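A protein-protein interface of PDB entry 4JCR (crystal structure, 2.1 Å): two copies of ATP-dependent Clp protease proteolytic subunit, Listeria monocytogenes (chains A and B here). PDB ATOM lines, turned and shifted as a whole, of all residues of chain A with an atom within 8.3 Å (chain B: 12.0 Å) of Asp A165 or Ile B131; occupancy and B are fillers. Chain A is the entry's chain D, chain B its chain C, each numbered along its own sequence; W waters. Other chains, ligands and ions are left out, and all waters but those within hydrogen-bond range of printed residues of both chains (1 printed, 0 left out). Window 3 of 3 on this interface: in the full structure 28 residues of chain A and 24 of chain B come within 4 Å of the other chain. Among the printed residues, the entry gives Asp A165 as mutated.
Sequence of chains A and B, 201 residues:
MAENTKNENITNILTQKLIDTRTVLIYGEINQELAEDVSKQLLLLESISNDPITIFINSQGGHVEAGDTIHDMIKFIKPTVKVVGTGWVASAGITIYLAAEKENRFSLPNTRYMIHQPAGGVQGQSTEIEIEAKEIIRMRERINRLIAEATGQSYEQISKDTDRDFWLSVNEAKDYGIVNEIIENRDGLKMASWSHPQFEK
OE1 of Glu B128 is in salt-bridge range of NE of Arg A164 (3.7 Å).
The side-chain carboxylate of Glu B135 is in salt-bridge range of the guanidinium group of Arg A112 (3.0 Å).
The side-chain carboxylate (OE2) of Glu B65 is in salt-bridge range of the guanidinium group (NH1) of Arg A112 (3.0 Å).
A ring nitrogen (ND1) of His A116 is in hydrogen-bond range of the side-chain carboxylate of Asp A165, at 2.9 Å.
CG2 of Ile B131 touches O of Asp A165, at 3.7 Å.
Trp A167 touches Glu B135.
Asp A165 touches just one residue of chain B: Ile B131 (3.7 Å).
Printed residues of chain A within 4 Å of Glu B65: Arg A112 (3.0 Å).
Printed residues of chain A within 4 Å of Glu B128: Arg A164 (3.7 Å).
Printed residues of chain B within 4 Å of Arg A112: Glu B65 and Glu B135.
Printed residues of chain A within 4 Å of Glu B135: Arg A112 (3.0 Å) and Trp A167 (3.2 Å).
Printed residues of chain B within 4 Å of Trp A167: Glu B135 (3.2 Å).
Ala B119 touches none of the printed residues of chain A.
The nearest printed residue of chain B that does not touch Arg A164 is Ile B131 (4.01 Å).
Hydrophobic or aromatic side chains of chain A that line the printed part of chain B: Trp A167.
Among the printed residues, Asp or Glu carboxylates within 4 Å of a Lys or Arg side-chain nitrogen of the other chain: Arg A112 with Glu B65 (3.0 Å), Arg A112 with Glu B135 (3.0 Å) and Arg A164 with Glu B128 (3.7 Å).
No position is printed for both chains.
Of the 5 pairs that touch across the chains among the printed residues, none has its exchanged pair printed and touching as well.
Water W1 lies within hydrogen-bond range of the side-chain carboxylate of Glu B65, the guanidinium group of Arg A112 and the side-chain sulfur of Met B139.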
ATOM      1  N   ALA A  90       6.859  25.338 -27.033  1.00  0.00           N
ATOM      2  CA  ALA A  90       6.646  24.547 -25.823  1.00  0.00           C
ATOM      3  C   ALA A  90       7.587  23.358 -25.727  1.00  0.00           C
ATOM      4  O   ALA A  90       7.968  22.774 -26.744  1.00  0.00           O
ATOM      5  CB  ALA A  90       5.197  24.082 -25.742  1.00  0.00           C
ATOM      6  N   SER A  91       7.962  23.019 -24.494  1.00  0.00           N
ATOM      7  CA  SER A  91       8.708  21.792 -24.189  1.00  0.00           C
ATOM      8  C   SER A  91      10.025  21.733 -24.969  1.00  0.00           C
ATOM      9  O   SER A  91      10.837  22.649 -24.857  1.00  0.00           O
ATOM     10  CB  SER A  91       7.824  20.561 -24.435  1.00  0.00           C
ATOM     11  OG  SER A  91       8.375  19.403 -23.835  1.00  0.00           O
ATOM     12  N   ARG A 112       2.325  31.921 -27.591  1.00  0.00           N
ATOM     13  CA  ARG A 112       2.400  31.517 -26.193  1.00  0.00           C
ATOM     14  C   ARG A 112       3.574  30.564 -25.949  1.00  0.00           C
ATOM     15  O   ARG A 112       4.057  29.902 -26.872  1.00  0.00           O
ATOM     16  CB  ARG A 112       1.068  30.956 -25.676  1.00  0.00           C
ATOM     17  CG  ARG A 112       0.373  29.951 -26.575  1.00  0.00           C
ATOM     18  CD  ARG A 112      -0.871  29.415 -25.884  1.00  0.00           C
ATOM     19  NE  ARG A 112      -1.503  28.337 -26.634  1.00  0.00           N
ATOM     20  CZ  ARG A 112      -2.132  27.301 -26.081  1.00  0.00           C
ATOM     21  NH1 ARG A 112      -2.682  26.374 -26.855  1.00  0.00           N
ATOM     22  NH2 ARG A 112      -2.209  27.181 -24.762  1.00  0.00           N
ATOM     23  N   TYR A 113       4.040  30.525 -24.706  1.00  0.00           N
ATOM     24  CA  TYR A 113       5.230  29.763 -24.342  1.00  0.00           C
ATOM     25  C   TYR A 113       4.915  28.809 -23.202  1.00  0.00           C
ATOM     26  O   TYR A 113       4.130  29.138 -22.315  1.00  0.00           O
ATOM     27  CB  TYR A 113       6.377  30.715 -23.967  1.00  0.00           C
ATOM     28  CG  TYR A 113       6.887  31.500 -25.157  1.00  0.00           C
ATOM     29  CD1 TYR A 113       8.044  31.110 -25.824  1.00  0.00           C
ATOM     30  CD2 TYR A 113       6.191  32.614 -25.638  1.00  0.00           C
ATOM     31  CE1 TYR A 113       8.508  31.810 -26.925  1.00  0.00           C
ATOM     32  CE2 TYR A 113       6.647  33.319 -26.743  1.00  0.00           C
ATOM     33  CZ  TYR A 113       7.804  32.908 -27.382  1.00  0.00           C
ATOM     34  OH  TYR A 113       8.262  33.595 -28.479  1.00  0.00           O
ATOM     35  N   MET A 114       5.507  27.620 -23.238  1.00  0.00           N
ATOM     36  CA  MET A 114       5.312  26.666 -22.154  1.00  0.00           C
ATOM     37  C   MET A 114       6.569  25.904 -21.787  1.00  0.00           C
ATOM     38  O   MET A 114       7.278  25.385 -22.651  1.00  0.00           O
ATOM     39  CB  MET A 114       4.178  25.687 -22.470  1.00  0.00           C
ATOM     40  CG  MET A 114       3.723  24.881 -21.261  1.00  0.00           C
ATOM     41  SD  MET A 114       4.035  23.100 -21.266  1.00  0.00           S
ATOM     42  CE  MET A 114       5.579  22.894 -22.134  1.00  0.00           C
ATOM     43  N   ILE A 115       6.817  25.827 -20.486  1.00  0.00           N
ATOM     44  CA  ILE A 115       7.825  24.933 -19.940  1.00  0.00           C
ATOM     45  C   ILE A 115       7.152  23.931 -19.007  1.00  0.00           C
ATOM     46  O   ILE A 115       6.141  24.238 -18.375  1.00  0.00           O
ATOM     47  CB  ILE A 115       8.951  25.700 -19.209  1.00  0.00           C
ATOM     48  CG1 ILE A 115       8.370  26.665 -18.162  1.00  0.00           C
ATOM     49  CG2 ILE A 115       9.821  26.431 -20.221  1.00  0.00           C
ATOM     50  CD1 ILE A 115       9.401  27.312 -17.259  1.00  0.00           C
ATOM     51  N   HIS A 116       7.700  22.723 -18.956  1.00  0.00           N
ATOM     52  CA  HIS A 116       7.218  21.676 -18.057  1.00  0.00           C
ATOM     53  C   HIS A 116       8.270  20.619 -17.916  1.00  0.00           C
ATOM     54  O   HIS A 116       9.300  20.672 -18.585  1.00  0.00           O
ATOM     55  CB  HIS A 116       5.892  21.084 -18.556  1.00  0.00           C
ATOM     56  CG  HIS A 116       6.019  20.215 -19.794  1.00  0.00           C
ATOM     57  ND1 HIS A 116       5.023  19.410 -20.211  1.00  0.00           N
ATOM     58  CD2 HIS A 116       7.069  20.037 -20.698  1.00  0.00           C
ATOM     59  CE1 HIS A 116       5.406  18.758 -21.327  1.00  0.00           C
ATOM     60  NE2 HIS A 116       6.656  19.139 -21.622  1.00  0.00           N
ATOM     61  N   GLN A 117       8.028  19.651 -17.042  1.00  0.00           N
ATOM     62  CA  GLN A 117       8.921  18.513 -16.919  1.00  0.00           C
ATOM     63  C   GLN A 117       8.421  17.400 -17.843  1.00  0.00           C
ATOM     64  O   GLN A 117       7.364  16.822 -17.598  1.00  0.00           O
ATOM     65  CB  GLN A 117       9.032  18.068 -15.458  1.00  0.00           C
ATOM     66  CG  GLN A 117       9.803  19.060 -14.593  1.00  0.00           C
ATOM     67  CD  GLN A 117       9.831  18.690 -13.122  1.00  0.00           C
ATOM     68  OE1 GLN A 117      10.039  17.530 -12.762  1.00  0.00           O
ATOM     69  NE2 GLN A 117       9.633  19.683 -12.261  1.00  0.00           N
ATOM     70  N   PRO A 118       9.169  17.122 -18.927  1.00  0.00           N
ATOM     71  CA  PRO A 118       8.750  16.175 -19.964  1.00  0.00           C
ATOM     72  C   PRO A 118       8.638  14.730 -19.477  1.00  0.00           C
ATOM     73  O   PRO A 118       9.270  14.352 -18.487  1.00  0.00           O
ATOM     74  CB  PRO A 118       9.864  16.288 -21.019  1.00  0.00           C
ATOM     75  CG  PRO A 118      10.533  17.592 -20.749  1.00  0.00           C
ATOM     76  CD  PRO A 118      10.463  17.747 -19.258  1.00  0.00           C
ATOM     77  N   ASP A 161       8.365  25.924 -10.940  1.00  0.00           N
ATOM     78  CA  ASP A 161       7.408  26.349 -11.969  1.00  0.00           C
ATOM     79  C   ASP A 161       7.056  25.259 -12.986  1.00  0.00           C
ATOM     80  O   ASP A 161       5.971  25.278 -13.562  1.00  0.00           O
ATOM     81  CB  ASP A 161       7.924  27.595 -12.696  1.00  0.00           C
ATOM     82  CG  ASP A 161       7.907  28.845 -11.818  1.00  0.00           C
ATOM     83  OD1 ASP A 161       7.123  28.896 -10.847  1.00  0.00           O
ATOM     84  OD2 ASP A 161       8.677  29.788 -12.109  1.00  0.00           O
ATOM     85  N   THR A 162       7.972  24.314 -13.201  1.00  0.00           N
ATOM     86  CA  THR A 162       7.776  23.246 -14.191  1.00  0.00           C
ATOM     87  C   THR A 162       7.096  21.993 -13.625  1.00  0.00           C
ATOM     88  O   THR A 162       7.010  20.973 -14.314  1.00  0.00           O
ATOM     89  CB  THR A 162       9.102  22.828 -14.863  1.00  0.00           C
ATOM     90  OG1 THR A 162      10.053  22.442 -13.863  1.00  0.00           O
ATOM     91  CG2 THR A 162       9.668  23.960 -15.707  1.00  0.00           C
ATOM     92  N   ASP A 163       6.616  22.071 -12.382  1.00  0.00           N
ATOM     93  CA  ASP A 163       5.941  20.941 -11.731  1.00  0.00           C
ATOM     94  C   ASP A 163       4.741  20.457 -12.548  1.00  0.00           C
ATOM     95  O   ASP A 163       4.505  19.253 -12.673  1.00  0.00           O
ATOM     96  CB  ASP A 163       5.509  21.311 -10.306  1.00  0.00           C
ATOM     97  CG  ASP A 163       4.995  20.113  -9.519  1.00  0.00           C
ATOM     98  OD1 ASP A 163       5.601  19.022  -9.612  1.00  0.00           O
ATOM     99  OD2 ASP A 163       3.983  20.264  -8.802  1.00  0.00           O
ATOM    100  N   ARG A 164       3.990  21.407 -13.098  1.00  0.00           N
ATOM    101  CA  ARG A 164       2.941  21.113 -14.070  1.00  0.00           C
ATOM    102  C   ARG A 164       3.109  22.002 -15.302  1.00  0.00           C
ATOM    103  O   ARG A 164       4.045  22.803 -15.364  1.00  0.00           O
ATOM    104  CB  ARG A 164       1.553  21.266 -13.439  1.00  0.00           C
ATOM    105  CG  ARG A 164       1.190  20.106 -12.522  1.00  0.00           C
ATOM    106  CD  ARG A 164      -0.297  20.039 -12.219  1.00  0.00           C
ATOM    107  NE  ARG A 164      -0.661  18.753 -11.624  1.00  0.00           N
ATOM    108  CZ  ARG A 164      -0.608  18.474 -10.322  1.00  0.00           C
ATOM    109  NH1 ARG A 164      -0.205  19.389  -9.448  1.00  0.00           N
ATOM    110  NH2 ARG A 164      -0.958  17.270  -9.891  1.00  0.00           N
ATOM    111  N   ASP A 165       2.219  21.850 -16.283  1.00  0.00           N
ATOM    112  CA  ASP A 165       2.285  22.636 -17.517  1.00  0.00           C
ATOM    113  C   ASP A 165       2.188  24.131 -17.224  1.00  0.00           C
ATOM    114  O   ASP A 165       1.163  24.612 -16.752  1.00  0.00           O
ATOM    115  CB  ASP A 165       1.192  22.201 -18.500  1.00  0.00           C
ATOM    116  CG  ASP A 165       1.524  20.896 -19.211  1.00  0.00           C
ATOM    117  OD1 ASP A 165       0.727  20.482 -20.075  1.00  0.00           O
ATOM    118  OD2 ASP A 165       2.575  20.284 -18.921  1.00  0.00           O
ATOM    119  N   PHE A 166       3.269  24.848 -17.517  1.00  0.00           N
ATOM    120  CA  PHE A 166       3.416  26.249 -17.137  1.00  0.00           C
ATOM    121  C   PHE A 166       3.370  27.159 -18.365  1.00  0.00           C
ATOM    122  O   PHE A 166       4.396  27.417 -19.002  1.00  0.00           O
ATOM    123  CB  PHE A 166       4.726  26.426 -16.352  1.00  0.00           C
ATOM    124  CG  PHE A 166       4.865  27.760 -15.674  1.00  0.00           C
ATOM    125  CD1 PHE A 166       4.015  28.126 -14.633  1.00  0.00           C
ATOM    126  CD2 PHE A 166       5.873  28.640 -16.056  1.00  0.00           C
ATOM    127  CE1 PHE A 166       4.152  29.355 -14.003  1.00  0.00           C
ATOM    128  CE2 PHE A 166       6.017  29.869 -15.428  1.00  0.00           C
ATOM    129  CZ  PHE A 166       5.156  30.228 -14.403  1.00  0.00           C
ATOM    130  N   TRP A 167       2.169  27.632 -18.690  1.00  0.00           N
ATOM    131  CA  TRP A 167       1.939  28.464 -19.871  1.00  0.00           C
ATOM    132  C   TRP A 167       2.132  29.927 -19.600  1.00  0.00           C
ATOM    133  O   TRP A 167       1.670  30.452 -18.588  1.00  0.00           O
ATOM    134  CB  TRP A 167       0.545  28.232 -20.437  1.00  0.00           C
ATOM    135  CG  TRP A 167       0.415  26.956 -21.231  1.00  0.00           C
ATOM    136  CD1 TRP A 167      -0.098  25.737 -20.800  1.00  0.00           C
ATOM    137  CD2 TRP A 167       0.812  26.730 -22.629  1.00  0.00           C
ATOM    138  NE1 TRP A 167      -0.046  24.802 -21.802  1.00  0.00           N
ATOM    139  CE2 TRP A 167       0.487  25.330 -22.925  1.00  0.00           C
ATOM    140  CE3 TRP A 167       1.385  27.516 -23.625  1.00  0.00           C
ATOM    141  CZ2 TRP A 167       0.730  24.765 -24.170  1.00  0.00           C
ATOM    142  CZ3 TRP A 167       1.627  26.932 -24.878  1.00  0.00           C
ATOM    143  CH2 TRP A 167       1.308  25.591 -25.141  1.00  0.00           C
ATOM    144  N   LEU A 168       2.812  30.592 -20.525  1.00  0.00           N
ATOM    145  CA  LEU A 168       3.091  32.017 -20.421  1.00  0.00           C
ATOM    146  C   LEU A 168       2.670  32.734 -21.693  1.00  0.00           C
ATOM    147  O   LEU A 168       2.958  32.268 -22.799  1.00  0.00           O
ATOM    148  CB  LEU A 168       4.585  32.255 -20.165  1.00  0.00           C
ATOM    149  CG  LEU A 168       5.207  31.668 -18.890  1.00  0.00           C
ATOM    150  CD1 LEU A 168       6.724  31.719 -18.956  1.00  0.00           C
ATOM    151  CD2 LEU A 168       4.697  32.377 -17.643  1.00  0.00           C
ATOM    152  N   GLU B  65      -2.695  28.026 -33.483  1.00  0.00           N
ATOM    153  CA  GLU B  65      -1.330  28.549 -33.496  1.00  0.00           C
ATOM    154  C   GLU B  65      -0.745  28.639 -34.906  1.00  0.00           C
ATOM    155  O   GLU B  65       0.096  29.496 -35.178  1.00  0.00           O
ATOM    156  CB  GLU B  65      -0.424  27.730 -32.573  1.00  0.00           C
ATOM    157  CG  GLU B  65      -0.689  27.956 -31.088  1.00  0.00           C
ATOM    158  CD  GLU B  65      -1.943  27.263 -30.577  1.00  0.00           C
ATOM    159  OE1 GLU B  65      -2.426  26.305 -31.223  1.00  0.00           O
ATOM    160  OE2 GLU B  65      -2.449  27.675 -29.513  1.00  0.00           O
ATOM    161  N   ALA B 119     -12.126  25.537 -30.209  1.00  0.00           N
ATOM    162  CA  ALA B 119     -11.737  24.510 -29.249  1.00  0.00           C
ATOM    163  C   ALA B 119     -10.229  24.518 -29.001  1.00  0.00           C
ATOM    164  O   ALA B 119      -9.467  25.095 -29.780  1.00  0.00           O
ATOM    165  CB  ALA B 119     -12.189  23.142 -29.741  1.00  0.00           C
ATOM    166  N   GLY B 120      -9.805  23.874 -27.915  1.00  0.00           N
ATOM    167  CA  GLY B 120      -8.387  23.810 -27.561  1.00  0.00           C
ATOM    168  C   GLY B 120      -7.867  22.397 -27.371  1.00  0.00           C
ATOM    169  O   GLY B 120      -8.231  21.717 -26.408  1.00  0.00           O
ATOM    170  N   GLU B 128      -4.869  19.249 -14.828  1.00  0.00           N
ATOM    171  CA  GLU B 128      -4.631  19.652 -16.213  1.00  0.00           C
ATOM    172  C   GLU B 128      -5.830  20.409 -16.781  1.00  0.00           C
ATOM    173  O   GLU B 128      -5.665  21.316 -17.596  1.00  0.00           O
ATOM    174  CB  GLU B 128      -4.341  18.428 -17.092  1.00  0.00           C
ATOM    175  CG  GLU B 128      -3.398  17.395 -16.486  1.00  0.00           C
ATOM    176  CD  GLU B 128      -1.989  17.918 -16.286  1.00  0.00           C
ATOM    177  OE1 GLU B 128      -1.598  18.136 -15.118  1.00  0.00           O
ATOM    178  OE2 GLU B 128      -1.275  18.113 -17.294  1.00  0.00           O
ATOM    179  N   ILE B 129      -7.031  20.024 -16.345  1.00  0.00           N
ATOM    180  CA  ILE B 129      -8.280  20.641 -16.804  1.00  0.00           C
ATOM    181  C   ILE B 129      -8.347  22.141 -16.487  1.00  0.00           C
ATOM    182  O   ILE B 129      -8.745  22.936 -17.340  1.00  0.00           O
ATOM    183  CB  ILE B 129      -9.523  19.873 -16.280  1.00  0.00           C
ATOM    184  CG1 ILE B 129      -9.932  18.771 -17.264  1.00  0.00           C
ATOM    185  CG2 ILE B 129     -10.710  20.799 -16.059  1.00  0.00           C
ATOM    186  CD1 ILE B 129      -9.077  17.522 -17.213  1.00  0.00           C
ATOM    187  N   GLU B 130      -7.936  22.515 -15.275  1.00  0.00           N
ATOM    188  CA  GLU B 130      -7.884  23.921 -14.864  1.00  0.00           C
ATOM    189  C   GLU B 130      -6.880  24.706 -15.704  1.00  0.00           C
ATOM    190  O   GLU B 130      -7.133  25.854 -16.078  1.00  0.00           O
ATOM    191  CB  GLU B 130      -7.530  24.042 -13.380  1.00  0.00           C
ATOM    192  CG  GLU B 130      -8.495  23.337 -12.441  1.00  0.00           C
ATOM    193  CD  GLU B 130      -8.144  23.543 -10.980  1.00  0.00           C
ATOM    194  OE1 GLU B 130      -8.267  24.686 -10.488  1.00  0.00           O
ATOM    195  OE2 GLU B 130      -7.760  22.556 -10.318  1.00  0.00           O
ATOM    196  N   ILE B 131      -5.742  24.074 -15.991  1.00  0.00           N
ATOM    197  CA  ILE B 131      -4.703  24.655 -16.842  1.00  0.00           C
ATOM    198  C   ILE B 131      -5.217  24.806 -18.276  1.00  0.00           C
ATOM    199  O   ILE B 131      -5.064  25.867 -18.883  1.00  0.00           O
ATOM    200  CB  ILE B 131      -3.400  23.819 -16.800  1.00  0.00           C
ATOM    201  CG1 ILE B 131      -2.805  23.830 -15.385  1.00  0.00           C
ATOM    202  CG2 ILE B 131      -2.382  24.340 -17.812  1.00  0.00           C
ATOM    203  CD1 ILE B 131      -1.743  22.776 -15.141  1.00  0.00           C
ATOM    204  N   GLU B 132      -5.841  23.749 -18.798  1.00  0.00           N
ATOM    205  CA  GLU B 132      -6.437  23.770 -20.136  1.00  0.00           C
ATOM    206  C   GLU B 132      -7.547  24.820 -20.241  1.00  0.00           C
ATOM    207  O   GLU B 132      -7.645  25.521 -21.248  1.00  0.00           O
ATOM    208  CB  GLU B 132      -6.966  22.381 -20.519  1.00  0.00           C
ATOM    209  CG  GLU B 132      -7.259  22.202 -22.006  1.00  0.00           C
ATOM    210  CD  GLU B 132      -7.652  20.780 -22.390  1.00  0.00           C
ATOM    211  OE1 GLU B 132      -7.983  19.966 -21.493  1.00  0.00           O
ATOM    212  OE2 GLU B 132      -7.633  20.471 -23.603  1.00  0.00           O
ATOM    213  N   ALA B 133      -8.364  24.931 -19.194  1.00  0.00           N
ATOM    214  CA  ALA B 133      -9.465  25.897 -19.153  1.00  0.00           C
ATOM    215  C   ALA B 133      -8.973  27.343 -19.166  1.00  0.00           C
ATOM    216  O   ALA B 133      -9.528  28.178 -19.879  1.00  0.00           O
ATOM    217  CB  ALA B 133     -10.361  25.649 -17.946  1.00  0.00           C
ATOM    218  N   LYS B 134      -7.934  27.632 -18.383  1.00  0.00           N
ATOM    219  CA  LYS B 134      -7.358  28.975 -18.344  1.00  0.00           C
ATOM    220  C   LYS B 134      -6.797  29.365 -19.711  1.00  0.00           C
ATOM    221  O   LYS B 134      -7.014  30.484 -20.179  1.00  0.00           O
ATOM    222  CB  LYS B 134      -6.271  29.088 -17.269  1.00  0.00           C
ATOM    223  CG  LYS B 134      -6.025  30.520 -16.802  1.00  0.00           C
ATOM    224  CD  LYS B 134      -4.732  30.671 -16.011  1.00  0.00           C
ATOM    225  CE  LYS B 134      -3.540  30.921 -16.925  1.00  0.00           C
ATOM    226  NZ  LYS B 134      -2.344  31.389 -16.170  1.00  0.00           N
ATOM    227  N   GLU B 135      -6.097  28.429 -20.350  1.00  0.00           N
ATOM    228  CA  GLU B 135      -5.488  28.659 -21.660  1.00  0.00           C
ATOM    229  C   GLU B 135      -6.501  28.964 -22.756  1.00  0.00           C
ATOM    230  O   GLU B 135      -6.275  29.848 -23.582  1.00  0.00           O
ATOM    231  CB  GLU B 135      -4.611  27.470 -22.066  1.00  0.00           C
ATOM    232  CG  GLU B 135      -3.255  27.456 -21.385  1.00  0.00           C
ATOM    233  CD  GLU B 135      -2.572  28.810 -21.443  1.00  0.00           C
ATOM    234  OE1 GLU B 135      -2.458  29.465 -20.382  1.00  0.00           O
ATOM    235  OE2 GLU B 135      -2.172  29.229 -22.552  1.00  0.00           O
ATOM    236  N   ILE B 136      -7.610  28.232 -22.759  1.00  0.00           N
ATOM    237  CA  ILE B 136      -8.649  28.420 -23.767  1.00  0.00           C
ATOM    238  C   ILE B 136      -9.407  29.736 -23.548  1.00  0.00           C
ATOM    239  O   ILE B 136      -9.860  30.363 -24.511  1.00  0.00           O
ATOM    240  CB  ILE B 136      -9.581  27.190 -23.843  1.00  0.00           C
ATOM    241  CG1 ILE B 136      -8.801  25.994 -24.399  1.00  0.00           C
ATOM    242  CG2 ILE B 136     -10.788  27.462 -24.730  1.00  0.00           C
ATOM    243  CD1 ILE B 136      -9.357  24.641 -24.008  1.00  0.00           C
ATOM    244  N   ILE B 137      -9.512  30.161 -22.288  1.00  0.00           N
ATOM    245  CA  ILE B 137     -10.106  31.457 -21.946  1.00  0.00           C
ATOM    246  C   ILE B 137      -9.254  32.609 -22.484  1.00  0.00           C
ATOM    247  O   ILE B 137      -9.767  33.488 -23.182  1.00  0.00           O
ATOM    248  CB  ILE B 137     -10.333  31.615 -20.419  1.00  0.00           C
ATOM    249  CG1 ILE B 137     -11.373  30.607 -19.905  1.00  0.00           C
ATOM    250  CG2 ILE B 137     -10.753  33.038 -20.065  1.00  0.00           C
ATOM    251  CD1 ILE B 137     -12.615  30.473 -20.764  1.00  0.00           C
ATOM    252  N   ARG B 138      -7.960  32.587 -22.164  1.00  0.00           N
ATOM    253  CA  ARG B 138      -7.018  33.612 -22.624  1.00  0.00           C
ATOM    254  C   ARG B 138      -6.948  33.660 -24.150  1.00  0.00           C
ATOM    255  O   ARG B 138      -6.933  34.741 -24.746  1.00  0.00           O
ATOM    256  CB  ARG B 138      -5.623  33.373 -22.041  1.00  0.00           C
ATOM    257  CG  ARG B 138      -5.570  33.388 -20.521  1.00  0.00           C
ATOM    258  CD  ARG B 138      -4.163  33.109 -20.015  1.00  0.00           C
ATOM    259  NE  ARG B 138      -3.375  34.334 -19.914  1.00  0.00           N
ATOM    260  CZ  ARG B 138      -2.075  34.378 -19.629  1.00  0.00           C
ATOM    261  NH1 ARG B 138      -1.389  33.262 -19.421  1.00  0.00           N
ATOM    262  NH2 ARG B 138      -1.458  35.549 -19.557  1.00  0.00           N
ATOM    263  N   MET B 139      -6.923  32.482 -24.769  1.00  0.00           N
ATOM    264  CA  MET B 139      -6.894  32.355 -26.223  1.00  0.00           C
ATOM    265  C   MET B 139      -8.129  32.972 -26.893  1.00  0.00           C
ATOM    266  O   MET B 139      -8.001  33.720 -27.865  1.00  0.00           O
ATOM    267  CB  MET B 139      -6.761  30.885 -26.613  1.00  0.00           C
ATOM    268  CG  MET B 139      -6.524  30.643 -28.091  1.00  0.00           C
ATOM    269  SD  MET B 139      -7.600  29.327 -28.686  1.00  0.00           S
ATOM    270  CE  MET B 139      -9.126  30.240 -28.858  1.00  0.00           C
ATOM    271  N   ARG B 140      -9.314  32.648 -26.375  1.00  0.00           N
ATOM    272  CA  ARG B 140     -10.578  33.184 -26.896  1.00  0.00           C
ATOM    273  C   ARG B 140     -10.651  34.699 -26.751  1.00  0.00           C
ATOM    274  O   ARG B 140     -11.155  35.394 -27.638  1.00  0.00           O
ATOM    275  CB  ARG B 140     -11.776  32.532 -26.200  1.00  0.00           C
ATOM    276  CG  ARG B 140     -12.148  31.179 -26.778  1.00  0.00           C
ATOM    277  CD  ARG B 140     -13.093  30.419 -25.865  1.00  0.00           C
ATOM    278  NE  ARG B 140     -13.383  29.091 -26.398  1.00  0.00           N
ATOM    279  CZ  ARG B 140     -14.086  28.154 -25.763  1.00  0.00           C
ATOM    280  NH1 ARG B 140     -14.584  28.384 -24.554  1.00  0.00           N
ATOM    281  NH2 ARG B 140     -14.282  26.979 -26.342  1.00  0.00           N
HETATM  282  O   HOH W   1      -4.923  27.755 -28.241  1.00  0.00           O
